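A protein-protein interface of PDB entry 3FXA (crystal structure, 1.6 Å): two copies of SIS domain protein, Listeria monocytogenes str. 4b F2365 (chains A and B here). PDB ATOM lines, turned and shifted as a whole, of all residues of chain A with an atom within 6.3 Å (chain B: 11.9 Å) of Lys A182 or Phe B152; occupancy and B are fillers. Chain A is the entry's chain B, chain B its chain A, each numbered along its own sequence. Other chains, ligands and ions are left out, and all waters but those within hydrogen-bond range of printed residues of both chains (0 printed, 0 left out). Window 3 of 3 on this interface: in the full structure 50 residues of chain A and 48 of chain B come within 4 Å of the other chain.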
ATOM      1  N   MET A 175      -6.798  -8.798  38.159  1.00  0.00           N
ATOM      2  CA  MET A 175      -7.343  -7.879  37.148  1.00  0.00           C
ATOM      3  C   MET A 175      -8.721  -7.337  37.588  1.00  0.00           C
ATOM      4  O   MET A 175      -8.991  -6.152  37.447  1.00  0.00           O
ATOM      5  CB  MET A 175      -7.415  -8.540  35.769  1.00  0.00           C
ATOM      6  CG  MET A 175      -6.054  -8.827  35.179  1.00  0.00           C
ATOM      7  SD  MET A 175      -6.196  -9.844  33.570  1.00  0.00           S
ATOM      8  CE  MET A 175      -7.087  -8.595  32.430  1.00  0.00           C
ATOM      9  N   TYR A 180      -8.335  -3.413  36.845  1.00  0.00           N
ATOM     10  CA  TYR A 180      -7.381  -3.196  35.752  1.00  0.00           C
ATOM     11  C   TYR A 180      -8.169  -2.883  34.486  1.00  0.00           C
ATOM     12  O   TYR A 180      -9.219  -3.505  34.235  1.00  0.00           O
ATOM     13  CB  TYR A 180      -6.457  -4.404  35.577  1.00  0.00           C
ATOM     14  CG  TYR A 180      -5.333  -4.203  34.578  1.00  0.00           C
ATOM     15  CD1 TYR A 180      -4.317  -3.275  34.822  1.00  0.00           C
ATOM     16  CD2 TYR A 180      -5.256  -4.977  33.411  1.00  0.00           C
ATOM     17  CE1 TYR A 180      -3.251  -3.090  33.903  1.00  0.00           C
ATOM     18  CE2 TYR A 180      -4.188  -4.809  32.495  1.00  0.00           C
ATOM     19  CZ  TYR A 180      -3.196  -3.860  32.754  1.00  0.00           C
ATOM     20  OH  TYR A 180      -2.155  -3.681  31.881  1.00  0.00           O
ATOM     21  N   THR A 181      -7.690  -1.888  33.733  1.00  0.00           N
ATOM     22  CA  THR A 181      -8.378  -1.387  32.550  1.00  0.00           C
ATOM     23  C   THR A 181      -7.639  -1.653  31.249  1.00  0.00           C
ATOM     24  O   THR A 181      -6.416  -1.872  31.221  1.00  0.00           O
ATOM     25  CB  THR A 181      -8.601   0.143  32.647  1.00  0.00           C
ATOM     26  OG1 THR A 181      -7.341   0.824  32.583  1.00  0.00           O
ATOM     27  CG2 THR A 181      -9.322   0.506  33.943  1.00  0.00           C
ATOM     28  N   LYS A 182      -8.412  -1.573  30.169  1.00  0.00           N
ATOM     29  CA  LYS A 182      -7.916  -1.712  28.799  1.00  0.00           C
ATOM     30  C   LYS A 182      -6.957  -0.570  28.441  1.00  0.00           C
ATOM     31  O   LYS A 182      -5.992  -0.799  27.730  1.00  0.00           O
ATOM     32  CB  LYS A 182      -9.095  -1.754  27.820  1.00  0.00           C
ATOM     33  CG  LYS A 182      -9.945  -3.010  27.986  1.00  0.00           C
ATOM     34  CD  LYS A 182      -9.527  -4.147  27.053  1.00  0.00           C
ATOM     35  CE  LYS A 182     -10.399  -4.198  25.805  1.00  0.00           C
ATOM     36  NZ  LYS A 182     -11.770  -4.702  26.149  1.00  0.00           N
ATOM     37  N   GLU A 183      -7.244   0.641  28.944  1.00  0.00           N
ATOM     38  CA  GLU A 183      -6.388   1.835  28.760  1.00  0.00           C
ATOM     39  C   GLU A 183      -4.970   1.576  29.298  1.00  0.00           C
ATOM     40  O   GLU A 183      -3.985   1.833  28.594  1.00  0.00           O
ATOM     41  CB  GLU A 183      -6.994   3.069  29.444  1.00  0.00           C
ATOM     42  CG  GLU A 183      -8.368   3.503  28.932  1.00  0.00           C
ATOM     43  N   GLN A 184      -4.883   1.063  30.530  1.00  0.00           N
ATOM     44  CA  GLN A 184      -3.597   0.667  31.147  1.00  0.00           C
ATOM     45  C   GLN A 184      -2.860  -0.396  30.327  1.00  0.00           C
ATOM     46  O   GLN A 184      -1.634  -0.321  30.161  1.00  0.00           O
ATOM     47  CB  GLN A 184      -3.806   0.112  32.553  1.00  0.00           C
ATOM     48  CG  GLN A 184      -4.144   1.121  33.611  1.00  0.00           C
ATOM     49  CD  GLN A 184      -4.411   0.427  34.939  1.00  0.00           C
ATOM     50  OE1 GLN A 184      -5.490  -0.123  35.159  1.00  0.00           O
ATOM     51  NE2 GLN A 184      -3.423   0.445  35.830  1.00  0.00           N
ATOM     52  N   PHE A 185      -3.614  -1.380  29.829  1.00  0.00           N
ATOM     53  CA  PHE A 185      -3.095  -2.458  28.983  1.00  0.00           C
ATOM     54  C   PHE A 185      -2.507  -1.908  27.687  1.00  0.00           C
ATOM     55  O   PHE A 185      -1.419  -2.323  27.293  1.00  0.00           O
ATOM     56  CB  PHE A 185      -4.226  -3.481  28.684  1.00  0.00           C
ATOM     57  CG  PHE A 185      -3.787  -4.716  27.914  1.00  0.00           C
ATOM     58  CD1 PHE A 185      -3.691  -4.682  26.507  1.00  0.00           C
ATOM     59  CD2 PHE A 185      -3.536  -5.918  28.577  1.00  0.00           C
ATOM     60  CE1 PHE A 185      -3.291  -5.828  25.778  1.00  0.00           C
ATOM     61  CE2 PHE A 185      -3.145  -7.073  27.865  1.00  0.00           C
ATOM     62  CZ  PHE A 185      -3.018  -7.022  26.457  1.00  0.00           C
ATOM     63  N   SER A 186      -3.215  -0.978  27.036  1.00  0.00           N
ATOM     64  CA  SER A 186      -2.757  -0.402  25.760  1.00  0.00           C
ATOM     65  C   SER A 186      -1.423   0.348  25.897  1.00  0.00           C
ATOM     66  O   SER A 186      -0.641   0.335  24.959  1.00  0.00           O
ATOM     67  CB  SER A 186      -3.810   0.490  25.090  1.00  0.00           C
ATOM     68  OG  SER A 186      -4.005   1.722  25.767  1.00  0.00           O
ATOM     69  N   VAL A 187      -1.191   0.983  27.051  1.00  0.00           N
ATOM     70  CA  VAL A 187       0.069   1.711  27.328  1.00  0.00           C
ATOM     71  C   VAL A 187       1.298   0.815  27.253  1.00  0.00           C
ATOM     72  O   VAL A 187       2.313   1.214  26.683  1.00  0.00           O
ATOM     73  CB  VAL A 187       0.058   2.383  28.747  1.00  0.00           C
ATOM     74  CG1 VAL A 187       1.455   2.895  29.160  1.00  0.00           C
ATOM     75  CG2 VAL A 187      -0.935   3.530  28.799  1.00  0.00           C
ATOM     76  N   ASN B  10     -13.387 -17.091  41.174  1.00  0.00           N
ATOM     77  CA  ASN B  10     -12.629 -16.504  40.028  1.00  0.00           C
ATOM     78  C   ASN B  10     -11.448 -17.411  39.629  1.00  0.00           C
ATOM     79  O   ASN B  10     -11.278 -17.771  38.440  1.00  0.00           O
ATOM     80  CB  ASN B  10     -12.177 -15.069  40.407  1.00  0.00           C
ATOM     81  CG  ASN B  10     -11.511 -14.305  39.255  1.00  0.00           C
ATOM     82  OD1 ASN B  10     -10.429 -14.667  38.776  1.00  0.00           O
ATOM     83  ND2 ASN B  10     -12.123 -13.203  38.858  1.00  0.00           N
ATOM     84  N   GLN B  13     -12.472 -20.884  38.105  1.00  0.00           N
ATOM     85  CA  GLN B  13     -12.929 -20.706  36.727  1.00  0.00           C
ATOM     86  C   GLN B  13     -11.705 -20.692  35.793  1.00  0.00           C
ATOM     87  O   GLN B  13     -11.689 -21.358  34.750  1.00  0.00           O
ATOM     88  CB  GLN B  13     -13.722 -19.404  36.580  1.00  0.00           C
ATOM     89  CG  GLN B  13     -14.352 -19.120  35.198  1.00  0.00           C
ATOM     90  CD  GLN B  13     -15.752 -19.687  35.002  1.00  0.00           C
ATOM     91  OE1 GLN B  13     -16.552 -19.104  34.271  1.00  0.00           O
ATOM     92  NE2 GLN B  13     -16.069 -20.787  35.675  1.00  0.00           N
ATOM     93  N   THR B  14     -10.656 -19.977  36.203  1.00  0.00           N
ATOM     94  CA  THR B  14      -9.426 -19.909  35.394  1.00  0.00           C
ATOM     95  C   THR B  14      -8.820 -21.300  35.209  1.00  0.00           C
ATOM     96  O   THR B  14      -8.488 -21.668  34.085  1.00  0.00           O
ATOM     97  CB  THR B  14      -8.378 -18.924  35.988  1.00  0.00           C
ATOM     98  OG1 THR B  14      -8.883 -17.588  35.878  1.00  0.00           O
ATOM     99  CG2 THR B  14      -7.055 -19.016  35.237  1.00  0.00           C
ATOM    100  N   GLU B  17     -10.851 -23.449  32.726  1.00  0.00           N
ATOM    101  CA  GLU B  17     -10.575 -23.060  31.333  1.00  0.00           C
ATOM    102  C   GLU B  17      -9.183 -23.506  30.854  1.00  0.00           C
ATOM    103  O   GLU B  17      -9.041 -23.971  29.712  1.00  0.00           O
ATOM    104  CB  GLU B  17     -10.805 -21.560  31.111  1.00  0.00           C
ATOM    105  CG  GLU B  17     -12.260 -21.132  31.330  1.00  0.00           C
ATOM    106  CD  GLU B  17     -12.538 -19.678  30.989  1.00  0.00           C
ATOM    107  OE1 GLU B  17     -11.958 -19.150  30.019  1.00  0.00           O
ATOM    108  OE2 GLU B  17     -13.385 -19.074  31.677  1.00  0.00           O
ATOM    109  N   LYS B 101       1.111 -16.418  18.459  1.00  0.00           N
ATOM    110  CA  LYS B 101      -0.322 -16.779  18.437  1.00  0.00           C
ATOM    111  C   LYS B 101      -0.983 -16.358  17.139  1.00  0.00           C
ATOM    112  O   LYS B 101      -1.486 -17.205  16.430  1.00  0.00           O
ATOM    113  CB  LYS B 101      -1.080 -16.200  19.640  1.00  0.00           C
ATOM    114  CG  LYS B 101      -2.536 -16.635  19.794  1.00  0.00           C
ATOM    115  CD  LYS B 101      -3.068 -16.010  21.082  1.00  0.00           C
ATOM    116  CE  LYS B 101      -4.528 -16.279  21.372  1.00  0.00           C
ATOM    117  NZ  LYS B 101      -5.443 -15.799  20.320  1.00  0.00           N
ATOM    118  N   VAL B 145      -6.661 -22.099  21.238  1.00  0.00           N
ATOM    119  CA  VAL B 145      -7.578 -22.194  22.381  1.00  0.00           C
ATOM    120  C   VAL B 145      -8.855 -21.432  22.029  1.00  0.00           C
ATOM    121  O   VAL B 145      -8.803 -20.397  21.345  1.00  0.00           O
ATOM    122  CB  VAL B 145      -6.925 -21.663  23.668  1.00  0.00           C
ATOM    123  CG1 VAL B 145      -5.660 -22.481  23.984  1.00  0.00           C
ATOM    124  CG2 VAL B 145      -6.564 -20.184  23.555  1.00  0.00           C
ATOM    125  N   SER B 146      -9.989 -21.974  22.468  1.00  0.00           N
ATOM    126  CA  SER B 146     -11.317 -21.406  22.199  1.00  0.00           C
ATOM    127  C   SER B 146     -11.840 -20.460  23.287  1.00  0.00           C
ATOM    128  O   SER B 146     -12.784 -19.706  23.032  1.00  0.00           O
ATOM    129  CB  SER B 146     -12.321 -22.548  22.026  1.00  0.00           C
ATOM    130  OG  SER B 146     -12.373 -23.364  23.186  1.00  0.00           O
ATOM    131  N   LYS B 147     -11.250 -20.527  24.483  1.00  0.00           N
ATOM    132  CA  LYS B 147     -11.667 -19.738  25.642  1.00  0.00           C
ATOM    133  C   LYS B 147     -10.444 -19.295  26.447  1.00  0.00           C
ATOM    134  O   LYS B 147      -9.662 -20.139  26.892  1.00  0.00           O
ATOM    135  CB  LYS B 147     -12.580 -20.579  26.529  1.00  0.00           C
ATOM    136  N   GLU B 148     -10.285 -17.980  26.610  1.00  0.00           N
ATOM    137  CA  GLU B 148      -9.200 -17.385  27.410  1.00  0.00           C
ATOM    138  C   GLU B 148      -9.821 -16.913  28.730  1.00  0.00           C
ATOM    139  O   GLU B 148     -10.808 -16.177  28.700  1.00  0.00           O
ATOM    140  CB  GLU B 148      -8.524 -16.231  26.668  1.00  0.00           C
ATOM    141  CG  GLU B 148      -7.450 -16.647  25.651  1.00  0.00           C
ATOM    142  CD  GLU B 148      -6.200 -17.251  26.295  1.00  0.00           C
ATOM    143  OE1 GLU B 148      -5.990 -17.111  27.523  1.00  0.00           O
ATOM    144  OE2 GLU B 148      -5.412 -17.875  25.572  1.00  0.00           O
ATOM    145  N   PRO B 149      -9.240 -17.312  29.887  1.00  0.00           N
ATOM    146  CA  PRO B 149      -9.869 -17.007  31.180  1.00  0.00           C
ATOM    147  C   PRO B 149      -9.884 -15.572  31.685  1.00  0.00           C
ATOM    148  O   PRO B 149     -10.681 -15.291  32.579  1.00  0.00           O
ATOM    149  CB  PRO B 149      -9.105 -17.906  32.157  1.00  0.00           C
ATOM    150  CG  PRO B 149      -7.817 -18.171  31.536  1.00  0.00           C
ATOM    151  CD  PRO B 149      -7.973 -18.047  30.066  1.00  0.00           C
ATOM    152  N   ASP B 150      -9.019 -14.697  31.156  1.00  0.00           N
ATOM    153  CA  ASP B 150      -8.950 -13.295  31.627  1.00  0.00           C
ATOM    154  C   ASP B 150     -10.167 -12.480  31.136  1.00  0.00           C
ATOM    155  O   ASP B 150     -10.658 -12.747  30.035  1.00  0.00           O
ATOM    156  CB  ASP B 150      -7.613 -12.633  31.247  1.00  0.00           C
ATOM    157  CG  ASP B 150      -7.527 -12.229  29.788  1.00  0.00           C
ATOM    158  OD1 ASP B 150      -8.006 -11.122  29.452  1.00  0.00           O
ATOM    159  OD2 ASP B 150      -6.909 -12.963  28.985  1.00  0.00           O
ATOM    160  N   PRO B 151     -10.646 -11.486  31.936  1.00  0.00           N
ATOM    161  CA  PRO B 151     -11.829 -10.669  31.547  1.00  0.00           C
ATOM    162  C   PRO B 151     -11.747  -9.953  30.178  1.00  0.00           C
ATOM    163  O   PRO B 151     -12.797  -9.724  29.551  1.00  0.00           O
ATOM    164  CB  PRO B 151     -11.976  -9.656  32.697  1.00  0.00           C
ATOM    165  CG  PRO B 151     -10.839  -9.868  33.608  1.00  0.00           C
ATOM    166  CD  PRO B 151     -10.220 -11.188  33.317  1.00  0.00           C
ATOM    167  N   PHE B 152     -10.535  -9.608  29.728  1.00  0.00           N
ATOM    168  CA  PHE B 152     -10.330  -8.964  28.413  1.00  0.00           C
ATOM    169  C   PHE B 152     -10.099  -9.903  27.226  1.00  0.00           C
ATOM    170  O   PHE B 152     -10.122  -9.425  26.088  1.00  0.00           O
ATOM    171  CB  PHE B 152      -9.154  -7.971  28.450  1.00  0.00           C
ATOM    172  CG  PHE B 152      -9.267  -6.893  29.496  1.00  0.00           C
ATOM    173  CD1 PHE B 152     -10.499  -6.281  29.799  1.00  0.00           C
ATOM    174  CD2 PHE B 152      -8.106  -6.404  30.109  1.00  0.00           C
ATOM    175  CE1 PHE B 152     -10.573  -5.263  30.746  1.00  0.00           C
ATOM    176  CE2 PHE B 152      -8.176  -5.377  31.050  1.00  0.00           C
ATOM    177  CZ  PHE B 152      -9.418  -4.808  31.363  1.00  0.00           C
ATOM    178  N   ASN B 153      -9.886 -11.206  27.471  1.00  0.00           N
ATOM    179  CA  ASN B 153      -9.561 -12.186  26.414  1.00  0.00           C
ATOM    180  C   ASN B 153      -8.219 -11.799  25.724  1.00  0.00           C
ATOM    181  O   ASN B 153      -8.038 -12.035  24.520  1.00  0.00           O
ATOM    182  CB  ASN B 153     -10.735 -12.282  25.406  1.00  0.00           C
ATOM    183  CG  ASN B 153     -10.812 -13.624  24.680  1.00  0.00           C
ATOM    184  OD1 ASN B 153     -11.271 -14.621  25.244  1.00  0.00           O
ATOM    185  ND2 ASN B 153     -10.451 -13.631  23.402  1.00  0.00           N
ATOM    186  N   MET B 154      -7.287 -11.237  26.516  1.00  0.00           N
ATOM    187  CA  MET B 154      -5.994 -10.667  26.059  1.00  0.00           C
ATOM    188  C   MET B 154      -4.675 -11.193  26.664  1.00  0.00           C
ATOM    189  O   MET B 154      -3.666 -11.192  25.955  1.00  0.00           O
ATOM    190  CB  MET B 154      -6.054  -9.134  26.224  1.00  0.00           C
ATOM    191  CG  MET B 154      -6.344  -8.381  24.931  1.00  0.00           C
ATOM    192  SD  MET B 154      -7.165  -6.640  25.131  1.00  0.00           S
ATOM    193  CE  MET B 154      -6.642  -6.140  26.934  1.00  0.00           C
ATOM    194  N   LEU B 155      -4.660 -11.600  27.938  1.00  0.00           N
ATOM    195  CA  LEU B 155      -3.430 -12.138  28.586  1.00  0.00           C
ATOM    196  C   LEU B 155      -2.792 -13.371  27.914  1.00  0.00           C
ATOM    197  O   LEU B 155      -1.594 -13.613  28.098  1.00  0.00           O
ATOM    198  CB  LEU B 155      -3.645 -12.462  30.084  1.00  0.00           C
ATOM    199  CG  LEU B 155      -3.426 -11.408  31.155  1.00  0.00           C
ATOM    200  CD1 LEU B 155      -3.689 -12.037  32.524  1.00  0.00           C
ATOM    201  CD2 LEU B 155      -2.010 -10.856  31.108  1.00  0.00           C
ATOM    202  N   ALA B 156      -3.595 -14.144  27.181  1.00  0.00           N
ATOM    203  CA  ALA B 156      -3.148 -15.347  26.478  1.00  0.00           C
ATOM    204  C   ALA B 156      -2.555 -16.441  27.405  1.00  0.00           C
ATOM    205  O   ALA B 156      -1.606 -17.112  27.035  1.00  0.00           O
ATOM    206  CB  ALA B 156      -2.170 -14.968  25.326  1.00  0.00           C
ATOM    207  N   THR B 157      -3.134 -16.622  28.597  1.00  0.00           N
ATOM    208  CA  THR B 157      -2.665 -17.603  29.595  1.00  0.00           C
ATOM    209  C   THR B 157      -2.945 -19.038  29.091  1.00  0.00           C
ATOM    210  O   THR B 157      -2.038 -19.872  29.019  1.00  0.00           O
ATOM    211  CB  THR B 157      -3.333 -17.380  30.985  1.00  0.00           C
ATOM    212  OG1 THR B 157      -4.751 -17.318  30.832  1.00  0.00           O
ATOM    213  CG2 THR B 157      -2.852 -16.076  31.655  1.00  0.00           C
ATOM    214  N   ALA B 158      -4.186 -19.313  28.722  1.00  0.00           N
ATOM    215  CA  ALA B 158      -4.530 -20.617  28.144  1.00  0.00           C
ATOM    216  C   ALA B 158      -3.730 -20.910  26.858  1.00  0.00           C
ATOM    217  O   ALA B 158      -3.217 -22.035  26.683  1.00  0.00           O
ATOM    218  CB  ALA B 158      -6.023 -20.715  27.864  1.00  0.00           C
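No position is printed for both chains.
Of the 8 pairs that touch across the chains among the printed residues, none has its exchanged pair printed and touching as well.
Hydrophobic or aromatic side chains of chain A that line the printed part of chain B: Met A175, Tyr A180 and Phe A185.
Hydrophobic or aromatic side chains of chain B within 4 Å of the printed part of chain A: Phe B152, Met B154 and Leu B155.
Among the printed residues, 8 pairs touch across the chains.
Among the printed residues, no Asp or Glu carboxylate lies within 4 Å of a Lys or Arg side-chain nitrogen of the other chain.
Of the printed residues of chain B, Met A175 touches Asp B150 (3.9 Å), Phe B152 (3.4 Å) and Leu B155 (3.5 Å).
No residue of chain B comes within 4 Å of Gln A184.
Of chain B, only Met B154 comes within 4 Å of Phe A185.
No residue of chain B comes within 4 Å of Ser A186.
Val B145 touches none of the printed residues of chain A.
Printed residues of chain A within 4 Å of Asp B150: Met A175 (3.9 Å).
Pro B151 touches none of the printed residues of chain A.
Phe B152 touches just these residues of chain A: Met A175 (3.4 Å), Tyr A180 (3.2 Å), Thr A181 (3.6 Å) and Lys A182 (3.6 Å).
Printed residues of chain A within 4 Å of Met B154: Lys A182 (3.5 Å) and Phe A185 (3.3 Å).
Of the printed residues of chain A, Leu B155 touches Met A175.
The nearest residue of chain B that does not touch Lys A182 is Pro B151 (6.2 Å).
The nearest printed residue of chain A that does not touch Asp B150 is Phe A185 (6.5 Å).
The backbone carbonyl oxygen (O) of Met A175 sits at hydrogen-bond distance from the backbone NH (N) of Tyr A180 (2.9 Å).
The side-chain hydroxyl (OH) of Tyr A180 sits close to the backbone NH (N) of Phe A185, 3.4 Å away.
The side-chain carboxylate (OD2) of Asp B150 is in hydrogen-bond range of the backbone NH (N) of Leu B155, at 2.8 Å.
N of Met B154 sits at hydrogen-bond distance from OD1 of Asp B150, 3.0 Å away.
The side-chain carboxylate (OD1) of Asp B150 sits at hydrogen-bond distance from the backbone NH (N) of Asn B153 (2.7 Å).
N of Phe B152 is in hydrogen-bond range of OD1 of Asp B150 (3.0 Å).
Met A175 touches Asp B150.
CE of Met A175 touches CD2 of Phe B152 (3.4 Å).
SD of Met A175 touches CD1 of Leu B155 (3.5 Å).
Phe B152 touches Tyr A180.
Phe B152 touches Thr A181.
Phe B152 touches Lys A182.
Lys A182 touches Met B154 (CD to CE, 3.5 Å).
Phe A185 touches Met B154.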
